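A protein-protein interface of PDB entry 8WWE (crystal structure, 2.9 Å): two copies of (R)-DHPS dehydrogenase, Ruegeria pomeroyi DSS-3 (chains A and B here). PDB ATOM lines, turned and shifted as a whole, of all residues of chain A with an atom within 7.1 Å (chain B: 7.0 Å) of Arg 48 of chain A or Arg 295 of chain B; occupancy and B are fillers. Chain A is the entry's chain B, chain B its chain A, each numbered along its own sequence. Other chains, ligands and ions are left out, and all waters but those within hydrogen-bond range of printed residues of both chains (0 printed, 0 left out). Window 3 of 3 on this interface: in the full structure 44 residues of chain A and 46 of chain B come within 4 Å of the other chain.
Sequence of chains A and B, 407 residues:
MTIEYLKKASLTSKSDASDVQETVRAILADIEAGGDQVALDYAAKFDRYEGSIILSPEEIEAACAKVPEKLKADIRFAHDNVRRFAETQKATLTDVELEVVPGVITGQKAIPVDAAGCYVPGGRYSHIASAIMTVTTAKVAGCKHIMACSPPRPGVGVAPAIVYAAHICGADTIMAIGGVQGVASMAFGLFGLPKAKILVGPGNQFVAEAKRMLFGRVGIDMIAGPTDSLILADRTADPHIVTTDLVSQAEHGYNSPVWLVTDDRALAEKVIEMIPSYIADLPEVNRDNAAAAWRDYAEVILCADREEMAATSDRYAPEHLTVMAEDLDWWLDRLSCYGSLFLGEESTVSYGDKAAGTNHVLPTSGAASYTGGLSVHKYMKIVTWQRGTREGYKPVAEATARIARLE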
ATOM      1  N   LYS A   7      19.663  -3.806  21.916  1.00  0.00           N
ATOM      2  CA  LYS A   7      18.595  -2.836  22.075  1.00  0.00           C
ATOM      3  C   LYS A   7      17.341  -3.661  22.292  1.00  0.00           C
ATOM      4  O   LYS A   7      17.081  -4.601  21.529  1.00  0.00           O
ATOM      5  CB  LYS A   7      18.498  -1.938  20.821  1.00  0.00           C
ATOM      6  CG  LYS A   7      17.888  -0.555  20.998  1.00  0.00           C
ATOM      7  CD  LYS A   7      16.385  -0.624  21.031  1.00  0.00           C
ATOM      8  CE  LYS A   7      15.784   0.733  21.261  1.00  0.00           C
ATOM      9  NZ  LYS A   7      14.358   0.500  21.553  1.00  0.00           N
ATOM     10  N   LYS A   8      16.539  -3.293  23.283  1.00  0.00           N
ATOM     11  CA  LYS A   8      15.287  -3.994  23.500  1.00  0.00           C
ATOM     12  C   LYS A   8      14.171  -2.994  23.260  1.00  0.00           C
ATOM     13  O   LYS A   8      14.349  -1.782  23.422  1.00  0.00           O
ATOM     14  CB  LYS A   8      15.177  -4.618  24.911  1.00  0.00           C
ATOM     15  CG  LYS A   8      16.344  -5.545  25.366  1.00  0.00           C
ATOM     16  CD  LYS A   8      16.034  -6.323  26.686  1.00  0.00           C
ATOM     17  CE  LYS A   8      17.154  -6.197  27.760  1.00  0.00           C
ATOM     18  NZ  LYS A   8      16.707  -6.395  29.194  1.00  0.00           N
ATOM     19  N   ALA A   9      13.044  -3.503  22.780  1.00  0.00           N
ATOM     20  CA  ALA A   9      11.869  -2.673  22.552  1.00  0.00           C
ATOM     21  C   ALA A   9      10.945  -2.702  23.753  1.00  0.00           C
ATOM     22  O   ALA A   9      10.861  -3.704  24.469  1.00  0.00           O
ATOM     23  CB  ALA A   9      11.123  -3.120  21.299  1.00  0.00           C
ATOM     24  N   SER A  10      10.248  -1.581  23.967  1.00  0.00           N
ATOM     25  CA  SER A  10       9.364  -1.470  25.115  1.00  0.00           C
ATOM     26  C   SER A  10       8.250  -2.514  25.045  1.00  0.00           C
ATOM     27  O   SER A  10       7.198  -2.312  24.423  1.00  0.00           O
ATOM     28  CB  SER A  10       8.803  -0.056  25.202  1.00  0.00           C
ATOM     29  OG  SER A  10       9.873   0.858  25.157  1.00  0.00           O
ATOM     30  N   LEU A  11       8.546  -3.644  25.695  1.00  0.00           N
ATOM     31  CA  LEU A  11       7.773  -4.876  25.771  1.00  0.00           C
ATOM     32  C   LEU A  11       7.305  -5.299  24.363  1.00  0.00           C
ATOM     33  O   LEU A  11       6.111  -5.347  24.031  1.00  0.00           O
ATOM     34  CB  LEU A  11       6.602  -4.729  26.757  1.00  0.00           C
ATOM     35  CG  LEU A  11       6.049  -6.040  27.365  1.00  0.00           C
ATOM     36  CD1 LEU A  11       7.117  -6.607  28.318  1.00  0.00           C
ATOM     37  CD2 LEU A  11       4.716  -5.979  28.107  1.00  0.00           C
ATOM     38  N   THR A  12       8.318  -5.518  23.501  1.00  0.00           N
ATOM     39  CA  THR A  12       8.224  -6.249  22.230  1.00  0.00           C
ATOM     40  C   THR A  12       9.331  -7.284  22.107  1.00  0.00           C
ATOM     41  O   THR A  12       9.283  -8.126  21.202  1.00  0.00           O
ATOM     42  CB  THR A  12       8.289  -5.271  21.041  1.00  0.00           C
ATOM     43  OG1 THR A  12       7.395  -4.174  21.264  1.00  0.00           O
ATOM     44  CG2 THR A  12       7.931  -5.954  19.719  1.00  0.00           C
ATOM     45  N   TYR A  42       0.021  -1.276  33.841  1.00  0.00           N
ATOM     46  CA  TYR A  42       0.370  -1.281  32.421  1.00  0.00           C
ATOM     47  C   TYR A  42       0.248   0.123  31.830  1.00  0.00           C
ATOM     48  O   TYR A  42       1.100   0.561  31.042  1.00  0.00           O
ATOM     49  CB  TYR A  42      -0.518  -2.258  31.659  1.00  0.00           C
ATOM     50  CG  TYR A  42      -0.081  -3.684  31.793  1.00  0.00           C
ATOM     51  CD1 TYR A  42       1.073  -4.122  31.152  1.00  0.00           C
ATOM     52  CD2 TYR A  42      -0.784  -4.591  32.592  1.00  0.00           C
ATOM     53  CE1 TYR A  42       1.510  -5.437  31.265  1.00  0.00           C
ATOM     54  CE2 TYR A  42      -0.356  -5.918  32.726  1.00  0.00           C
ATOM     55  CZ  TYR A  42       0.800  -6.324  32.052  1.00  0.00           C
ATOM     56  OH  TYR A  42       1.291  -7.604  32.130  1.00  0.00           O
ATOM     57  N   ALA A  43      -0.790   0.857  32.244  1.00  0.00           N
ATOM     58  CA  ALA A  43      -1.019   2.206  31.743  1.00  0.00           C
ATOM     59  C   ALA A  43       0.189   3.087  32.022  1.00  0.00           C
ATOM     60  O   ALA A  43       0.782   3.658  31.102  1.00  0.00           O
ATOM     61  CB  ALA A  43      -2.285   2.798  32.376  1.00  0.00           C
ATOM     62  N   ALA A  44       0.543   3.225  33.303  1.00  0.00           N
ATOM     63  CA  ALA A  44       1.746   3.951  33.701  1.00  0.00           C
ATOM     64  C   ALA A  44       2.962   3.467  32.920  1.00  0.00           C
ATOM     65  O   ALA A  44       3.730   4.275  32.386  1.00  0.00           O
ATOM     66  CB  ALA A  44       1.954   3.839  35.213  1.00  0.00           C
ATOM     67  N   LYS A  45       3.179   2.149  32.881  1.00  0.00           N
ATOM     68  CA  LYS A  45       4.387   1.598  32.259  1.00  0.00           C
ATOM     69  C   LYS A  45       4.541   2.029  30.805  1.00  0.00           C
ATOM     70  O   LYS A  45       5.597   2.546  30.408  1.00  0.00           O
ATOM     71  CB  LYS A  45       4.393   0.073  32.367  1.00  0.00           C
ATOM     72  CG  LYS A  45       5.583  -0.573  31.670  1.00  0.00           C
ATOM     73  CD  LYS A  45       6.028  -1.824  32.401  1.00  0.00           C
ATOM     74  CE  LYS A  45       7.127  -2.557  31.657  1.00  0.00           C
ATOM     75  NZ  LYS A  45       6.687  -2.956  30.314  1.00  0.00           N
ATOM     76  N   PHE A  46       3.498   1.796  29.991  1.00  0.00           N
ATOM     77  CA  PHE A  46       3.554   1.927  28.534  1.00  0.00           C
ATOM     78  C   PHE A  46       3.222   3.332  28.064  1.00  0.00           C
ATOM     79  O   PHE A  46       3.892   3.876  27.181  1.00  0.00           O
ATOM     80  CB  PHE A  46       2.563   1.005  27.856  1.00  0.00           C
ATOM     81  CG  PHE A  46       2.796  -0.399  28.106  1.00  0.00           C
ATOM     82  CD1 PHE A  46       1.726  -1.243  28.339  1.00  0.00           C
ATOM     83  CD2 PHE A  46       4.081  -0.911  28.089  1.00  0.00           C
ATOM     84  CE1 PHE A  46       1.917  -2.579  28.552  1.00  0.00           C
ATOM     85  CE2 PHE A  46       4.285  -2.262  28.317  1.00  0.00           C
ATOM     86  CZ  PHE A  46       3.193  -3.096  28.554  1.00  0.00           C
ATOM     87  N   ASP A  47       2.146   3.892  28.634  1.00  0.00           N
ATOM     88  CA  ASP A  47       1.724   5.232  28.304  1.00  0.00           C
ATOM     89  C   ASP A  47       2.578   6.252  29.029  1.00  0.00           C
ATOM     90  O   ASP A  47       2.859   7.319  28.453  1.00  0.00           O
ATOM     91  CB  ASP A  47       0.254   5.479  28.646  1.00  0.00           C
ATOM     92  CG  ASP A  47      -0.716   4.644  27.816  1.00  0.00           C
ATOM     93  OD1 ASP A  47      -0.404   4.300  26.636  1.00  0.00           O
ATOM     94  OD2 ASP A  47      -1.793   4.323  28.362  1.00  0.00           O
ATOM     95  N   ARG A  48       3.019   5.962  30.277  1.00  0.00           N
ATOM     96  CA  ARG A  48       3.805   6.995  30.957  1.00  0.00           C
ATOM     97  C   ARG A  48       3.125   8.359  31.002  1.00  0.00           C
ATOM     98  O   ARG A  48       3.579   9.338  30.416  1.00  0.00           O
ATOM     99  CB  ARG A  48       5.252   7.050  30.466  1.00  0.00           C
ATOM    100  CG  ARG A  48       6.206   5.904  30.131  1.00  0.00           C
ATOM    101  CD  ARG A  48       6.894   6.242  28.915  1.00  0.00           C
ATOM    102  NE  ARG A  48       7.662   7.396  28.626  1.00  0.00           N
ATOM    103  CZ  ARG A  48       7.077   8.021  27.589  1.00  0.00           C
ATOM    104  NH1 ARG A  48       6.112   7.290  26.894  1.00  0.00           N
ATOM    105  NH2 ARG A  48       7.496   9.192  27.084  1.00  0.00           N
ATOM    106  N   TYR A  49       2.030   8.379  31.751  1.00  0.00           N
ATOM    107  CA  TYR A  49       1.168   9.526  31.926  1.00  0.00           C
ATOM    108  C   TYR A  49       0.645   9.438  33.339  1.00  0.00           C
ATOM    109  O   TYR A  49       0.186   8.380  33.780  1.00  0.00           O
ATOM    110  CB  TYR A  49       0.032   9.603  30.885  1.00  0.00           C
ATOM    111  CG  TYR A  49      -1.092  10.534  31.282  1.00  0.00           C
ATOM    112  CD1 TYR A  49      -0.973  11.915  31.125  1.00  0.00           C
ATOM    113  CD2 TYR A  49      -2.275  10.022  31.798  1.00  0.00           C
ATOM    114  CE1 TYR A  49      -2.005  12.760  31.486  1.00  0.00           C
ATOM    115  CE2 TYR A  49      -3.318  10.841  32.149  1.00  0.00           C
ATOM    116  CZ  TYR A  49      -3.186  12.213  31.996  1.00  0.00           C
ATOM    117  OH  TYR A  49      -4.254  13.015  32.362  1.00  0.00           O
ATOM    118  N   GLU A  50       0.710  10.585  34.009  1.00  0.00           N
ATOM    119  CA  GLU A  50       0.673  10.756  35.452  1.00  0.00           C
ATOM    120  C   GLU A  50      -0.654  11.350  35.917  1.00  0.00           C
ATOM    121  O   GLU A  50      -0.821  11.627  37.109  1.00  0.00           O
ATOM    122  CB  GLU A  50       1.853  11.680  35.814  1.00  0.00           C
ATOM    123  CG  GLU A  50       3.306  11.152  35.483  1.00  0.00           C
ATOM    124  CD  GLU A  50       3.963  10.205  36.503  1.00  0.00           C
ATOM    125  OE1 GLU A  50       3.820  10.479  37.722  1.00  0.00           O
ATOM    126  OE2 GLU A  50       4.601   9.197  36.099  1.00  0.00           O
ATOM    127  N   GLY A  51      -1.620  11.502  35.003  1.00  0.00           N
ATOM    128  CA  GLY A  51      -2.955  11.944  35.342  1.00  0.00           C
ATOM    129  C   GLY A  51      -3.993  10.831  35.417  1.00  0.00           C
ATOM    130  O   GLY A  51      -3.725   9.663  35.154  1.00  0.00           O
ATOM    131  N   PRO A 152      -3.005   8.686  26.380  1.00  0.00           N
ATOM    132  CA  PRO A 152      -2.550  10.021  26.780  1.00  0.00           C
ATOM    133  C   PRO A 152      -1.119  10.237  26.337  1.00  0.00           C
ATOM    134  O   PRO A 152      -0.301   9.315  26.293  1.00  0.00           O
ATOM    135  CB  PRO A 152      -2.669   9.980  28.304  1.00  0.00           C
ATOM    136  CG  PRO A 152      -2.424   8.561  28.627  1.00  0.00           C
ATOM    137  CD  PRO A 152      -3.063   7.766  27.529  1.00  0.00           C
ATOM    138  N   ARG A 153      -0.818  11.472  26.027  1.00  0.00           N
ATOM    139  CA  ARG A 153       0.532  11.893  25.678  1.00  0.00           C
ATOM    140  C   ARG A 153       1.155  12.517  26.925  1.00  0.00           C
ATOM    141  O   ARG A 153       0.429  13.120  27.745  1.00  0.00           O
ATOM    142  CB  ARG A 153       0.474  12.846  24.488  1.00  0.00           C
ATOM    143  CG  ARG A 153       1.716  13.539  24.039  1.00  0.00           C
ATOM    144  CD  ARG A 153       1.534  14.104  22.619  1.00  0.00           C
ATOM    145  NE  ARG A 153       1.698  13.087  21.567  1.00  0.00           N
ATOM    146  CZ  ARG A 153       2.867  12.552  21.195  1.00  0.00           C
ATOM    147  NH1 ARG A 153       2.922  11.628  20.238  1.00  0.00           N
ATOM    148  NH2 ARG A 153       3.990  12.954  21.768  1.00  0.00           N
ATOM    149  N   PRO A 154       2.452  12.347  27.194  1.00  0.00           N
ATOM    150  CA  PRO A 154       2.973  12.661  28.539  1.00  0.00           C
ATOM    151  C   PRO A 154       2.786  14.123  28.917  1.00  0.00           C
ATOM    152  O   PRO A 154       3.149  15.037  28.170  1.00  0.00           O
ATOM    153  CB  PRO A 154       4.456  12.292  28.429  1.00  0.00           C
ATOM    154  CG  PRO A 154       4.761  12.312  26.973  1.00  0.00           C
ATOM    155  CD  PRO A 154       3.514  11.842  26.298  1.00  0.00           C
ATOM    156  N   GLY A 155       2.213  14.335  30.094  1.00  0.00           N
ATOM    157  CA  GLY A 155       1.925  15.663  30.605  1.00  0.00           C
ATOM    158  C   GLY A 155       0.716  16.348  29.989  1.00  0.00           C
ATOM    159  O   GLY A 155       0.079  17.193  30.631  1.00  0.00           O
ATOM    160  N   ILE B 279      16.891  10.453  12.862  1.00  0.00           N
ATOM    161  CA  ILE B 279      15.576  10.874  13.333  1.00  0.00           C
ATOM    162  C   ILE B 279      15.404  12.387  13.208  1.00  0.00           C
ATOM    163  O   ILE B 279      14.327  12.877  12.837  1.00  0.00           O
ATOM    164  CB  ILE B 279      15.385  10.413  14.783  1.00  0.00           C
ATOM    165  CG1 ILE B 279      15.196   8.901  14.830  1.00  0.00           C
ATOM    166  CG2 ILE B 279      14.218  11.150  15.421  1.00  0.00           C
ATOM    167  CD1 ILE B 279      14.955   8.390  16.216  1.00  0.00           C
ATOM    168  N   ALA B 290       8.672   8.823  14.954  1.00  0.00           N
ATOM    169  CA  ALA B 290       9.848   7.994  14.675  1.00  0.00           C
ATOM    170  C   ALA B 290      10.658   7.707  15.926  1.00  0.00           C
ATOM    171  O   ALA B 290      11.117   6.579  16.110  1.00  0.00           O
ATOM    172  CB  ALA B 290      10.717   8.672  13.607  1.00  0.00           C
ATOM    173  N   ALA B 291      10.971   8.741  16.720  1.00  0.00           N
ATOM    174  CA  ALA B 291      11.698   8.504  17.968  1.00  0.00           C
ATOM    175  C   ALA B 291      10.948   7.505  18.850  1.00  0.00           C
ATOM    176  O   ALA B 291      11.531   6.523  19.357  1.00  0.00           O
ATOM    177  CB  ALA B 291      11.938   9.821  18.710  1.00  0.00           C
ATOM    178  N   ALA B 292       9.641   7.744  19.025  1.00  0.00           N
ATOM    179  CA  ALA B 292       8.816   6.857  19.836  1.00  0.00           C
ATOM    180  C   ALA B 292       8.904   5.429  19.318  1.00  0.00           C
ATOM    181  O   ALA B 292       9.176   4.491  20.080  1.00  0.00           O
ATOM    182  CB  ALA B 292       7.365   7.335  19.850  1.00  0.00           C
ATOM    183  N   ALA B 293       8.675   5.256  18.009  1.00  0.00           N
ATOM    184  CA  ALA B 293       8.711   3.945  17.372  1.00  0.00           C
ATOM    185  C   ALA B 293      10.061   3.271  17.573  1.00  0.00           C
ATOM    186  O   ALA B 293      10.117   2.087  17.893  1.00  0.00           O
ATOM    187  CB  ALA B 293       8.361   4.047  15.885  1.00  0.00           C
ATOM    188  N   TRP B 294      11.168   3.986  17.358  1.00  0.00           N
ATOM    189  CA  TRP B 294      12.462   3.331  17.523  1.00  0.00           C
ATOM    190  C   TRP B 294      12.588   2.753  18.917  1.00  0.00           C
ATOM    191  O   TRP B 294      12.818   1.554  19.078  1.00  0.00           O
ATOM    192  CB  TRP B 294      13.635   4.261  17.252  1.00  0.00           C
ATOM    193  CG  TRP B 294      14.950   3.640  17.678  1.00  0.00           C
ATOM    194  CD1 TRP B 294      15.643   3.916  18.817  1.00  0.00           C
ATOM    195  CD2 TRP B 294      15.721   2.640  16.973  1.00  0.00           C
ATOM    196  NE1 TRP B 294      16.798   3.168  18.866  1.00  0.00           N
ATOM    197  CE2 TRP B 294      16.870   2.375  17.749  1.00  0.00           C
ATOM    198  CE3 TRP B 294      15.557   1.959  15.762  1.00  0.00           C
ATOM    199  CZ2 TRP B 294      17.850   1.448  17.355  1.00  0.00           C
ATOM    200  CZ3 TRP B 294      16.535   1.032  15.375  1.00  0.00           C
ATOM    201  CH2 TRP B 294      17.664   0.790  16.173  1.00  0.00           C
ATOM    202  N   ARG B 295      12.388   3.578  19.950  1.00  0.00           N
ATOM    203  CA  ARG B 295      12.575   3.027  21.296  1.00  0.00           C
ATOM    204  C   ARG B 295      11.572   1.911  21.596  1.00  0.00           C
ATOM    205  O   ARG B 295      11.872   0.973  22.341  1.00  0.00           O
ATOM    206  CB  ARG B 295      12.494   4.099  22.376  1.00  0.00           C
ATOM    207  CG  ARG B 295      11.115   4.550  22.621  1.00  0.00           C
ATOM    208  CD  ARG B 295      10.887   5.224  23.929  1.00  0.00           C
ATOM    209  NE  ARG B 295       9.575   5.845  23.820  1.00  0.00           N
ATOM    210  CZ  ARG B 295       8.906   6.428  24.802  1.00  0.00           C
ATOM    211  NH1 ARG B 295       7.718   6.956  24.536  1.00  0.00           N
ATOM    212  NH2 ARG B 295       9.414   6.489  26.031  1.00  0.00           N
ATOM    213  N   ASP B 296      10.368   2.016  21.052  1.00  0.00           N
ATOM    214  CA  ASP B 296       9.233   1.264  21.546  1.00  0.00           C
ATOM    215  C   ASP B 296       8.997  -0.046  20.770  1.00  0.00           C
ATOM    216  O   ASP B 296       8.453  -1.015  21.325  1.00  0.00           O
ATOM    217  CB  ASP B 296       8.083   2.295  21.634  1.00  0.00           C
ATOM    218  CG  ASP B 296       6.904   1.844  22.484  1.00  0.00           C
ATOM    219  OD1 ASP B 296       6.762   0.603  22.732  1.00  0.00           O
ATOM    220  OD2 ASP B 296       6.236   2.788  23.046  1.00  0.00           O
ATOM    221  N   TYR B 297       9.357  -0.094  19.482  1.00  0.00           N
ATOM    222  CA  TYR B 297       9.072  -1.217  18.579  1.00  0.00           C
ATOM    223  C   TYR B 297      10.317  -1.877  17.979  1.00  0.00           C
ATOM    224  O   TYR B 297      10.208  -2.998  17.465  1.00  0.00           O
ATOM    225  CB  TYR B 297       8.102  -0.786  17.456  1.00  0.00           C
ATOM    226  CG  TYR B 297       6.721  -0.489  18.003  1.00  0.00           C
ATOM    227  CD1 TYR B 297       5.916  -1.509  18.496  1.00  0.00           C
ATOM    228  CD2 TYR B 297       6.237   0.812  18.066  1.00  0.00           C
ATOM    229  CE1 TYR B 297       4.648  -1.251  19.013  1.00  0.00           C
ATOM    230  CE2 TYR B 297       4.972   1.084  18.585  1.00  0.00           C
ATOM    231  CZ  TYR B 297       4.185   0.051  19.053  1.00  0.00           C
ATOM    232  OH  TYR B 297       2.934   0.317  19.560  1.00  0.00           O
ATOM    233  N   ALA B 298      11.474  -1.185  17.955  1.00  0.00           N
ATOM    234  CA  ALA B 298      12.730  -1.646  17.345  1.00  0.00           C
ATOM    235  C   ALA B 298      13.622  -2.410  18.320  1.00  0.00           C
ATOM    236  O   ALA B 298      13.714  -2.048  19.490  1.00  0.00           O
ATOM    237  CB  ALA B 298      13.512  -0.462  16.779  1.00  0.00           C
ATOM    238  N   GLU B 299      14.285  -3.468  17.836  1.00  0.00           N
ATOM    239  CA  GLU B 299      15.235  -4.235  18.645  1.00  0.00           C
ATOM    240  C   GLU B 299      16.484  -4.592  17.852  1.00  0.00           C
ATOM    241  O   GLU B 299      16.410  -4.873  16.658  1.00  0.00           O
ATOM    242  CB  GLU B 299      14.657  -5.555  19.180  1.00  0.00           C
ATOM    243  CG  GLU B 299      13.251  -5.529  19.726  1.00  0.00           C
ATOM    244  CD  GLU B 299      12.836  -6.890  20.269  1.00  0.00           C
ATOM    245  OE1 GLU B 299      13.677  -7.587  20.867  1.00  0.00           O
ATOM    246  OE2 GLU B 299      11.682  -7.302  20.019  1.00  0.00           O
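Of chain B, only Arg 295 (2.9 Å) comes within 4 Å of Arg 48 of chain A.
Of chain A, only Lys 7 (2.7 Å), Lys 8 (3.9 Å), Ala 9 (3.7 Å), Ser 10 (3.4 Å) and Arg 48 (2.9 Å) come within 4 Å of Arg 295 of chain B.
Printed residues of chain B within 4 Å of Ser 10 of chain A: Arg 295 and Asp 296.
Of the printed residues of chain A, Asp 296 of chain B touches Ala 9 (3.4 Å), Ser 10 (3.2 Å) and Thr 12 (3.3 Å).
Printed residues of chain B within 4 Å of Lys 7 of chain A: Trp 294, Arg 295, Ala 298 and Glu 299.
The nearest residue of chain A that does not touch Arg 295 of chain B is Phe 46 of chain A (5.6 Å).
The nearest printed residue of chain A that does not touch Trp 294 of chain B is Ala 9 of chain A (5.4 Å).
Hydrophobic or aromatic side chains of chain A that line the printed part of chain B: Ala 9.
Among the printed residues, no Asp or Glu carboxylate lies within 4 Å of a Lys or Arg side-chain nitrogen of the other chain.
The backbone NH (N) of Arg 48 of chain A sits at hydrogen-bond distance from the backbone carbonyl oxygen (O) of Ala 43 of chain A.
O of Arg 295 of chain B lies within hydrogen-bond range of N of Ser 10 of chain A (3.4 Å).
The backbone carbonyl oxygen (O) of Trp 294 of chain B is in hydrogen-bond range of the side-chain amino group (NZ) of Lys 7 of chain A.
The guanidinium group of Arg 48 of chain A sits close to the guanidinium group of Arg 295 of chain B, 2.9 Å away.
NZ of Lys 7 of chain A is in hydrogen-bond range of O of Arg 295 of chain B, 2.7 Å away.
O of Ala 298 of chain B is in hydrogen-bond range of NZ of Lys 7 of chain A, 3.3 Å away.
The backbone carbonyl oxygen (O) of Asp 296 of chain B sits at hydrogen-bond distance from the side-chain hydroxyl (OG1) of Thr 12 of chain A, at 3.3 Å.
The backbone carbonyl oxygen (O) of Thr 12 of chain A lies close to the side-chain carboxylate (OE2) of Glu 299 of chain B.
O of Asp 296 of chain B sits at hydrogen-bond distance from N of Ser 10 of chain A, at 3.2 Å.
No position is printed for both chains.
Of the 16 pairs that touch across the chains among the printed residues, none has its exchanged pair printed and touching as well.
Among the printed residues, merely in contact across the chains: Ala 9 of chain A with Ala 298 of chain B, Ala 9 of chain A with Asp 296 of chain B, Lys 7 of chain A with Glu 299 of chain B, Ala 9 of chain A with Glu 299 of chain B, Ala 9 of chain A with Tyr 297 of chain B, Ala 9 of chain A with Arg 295 of chain B, Lys 8 of chain A with Arg 295 of chain B and Lys 8 of chain A with Ala 298 of chain B.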
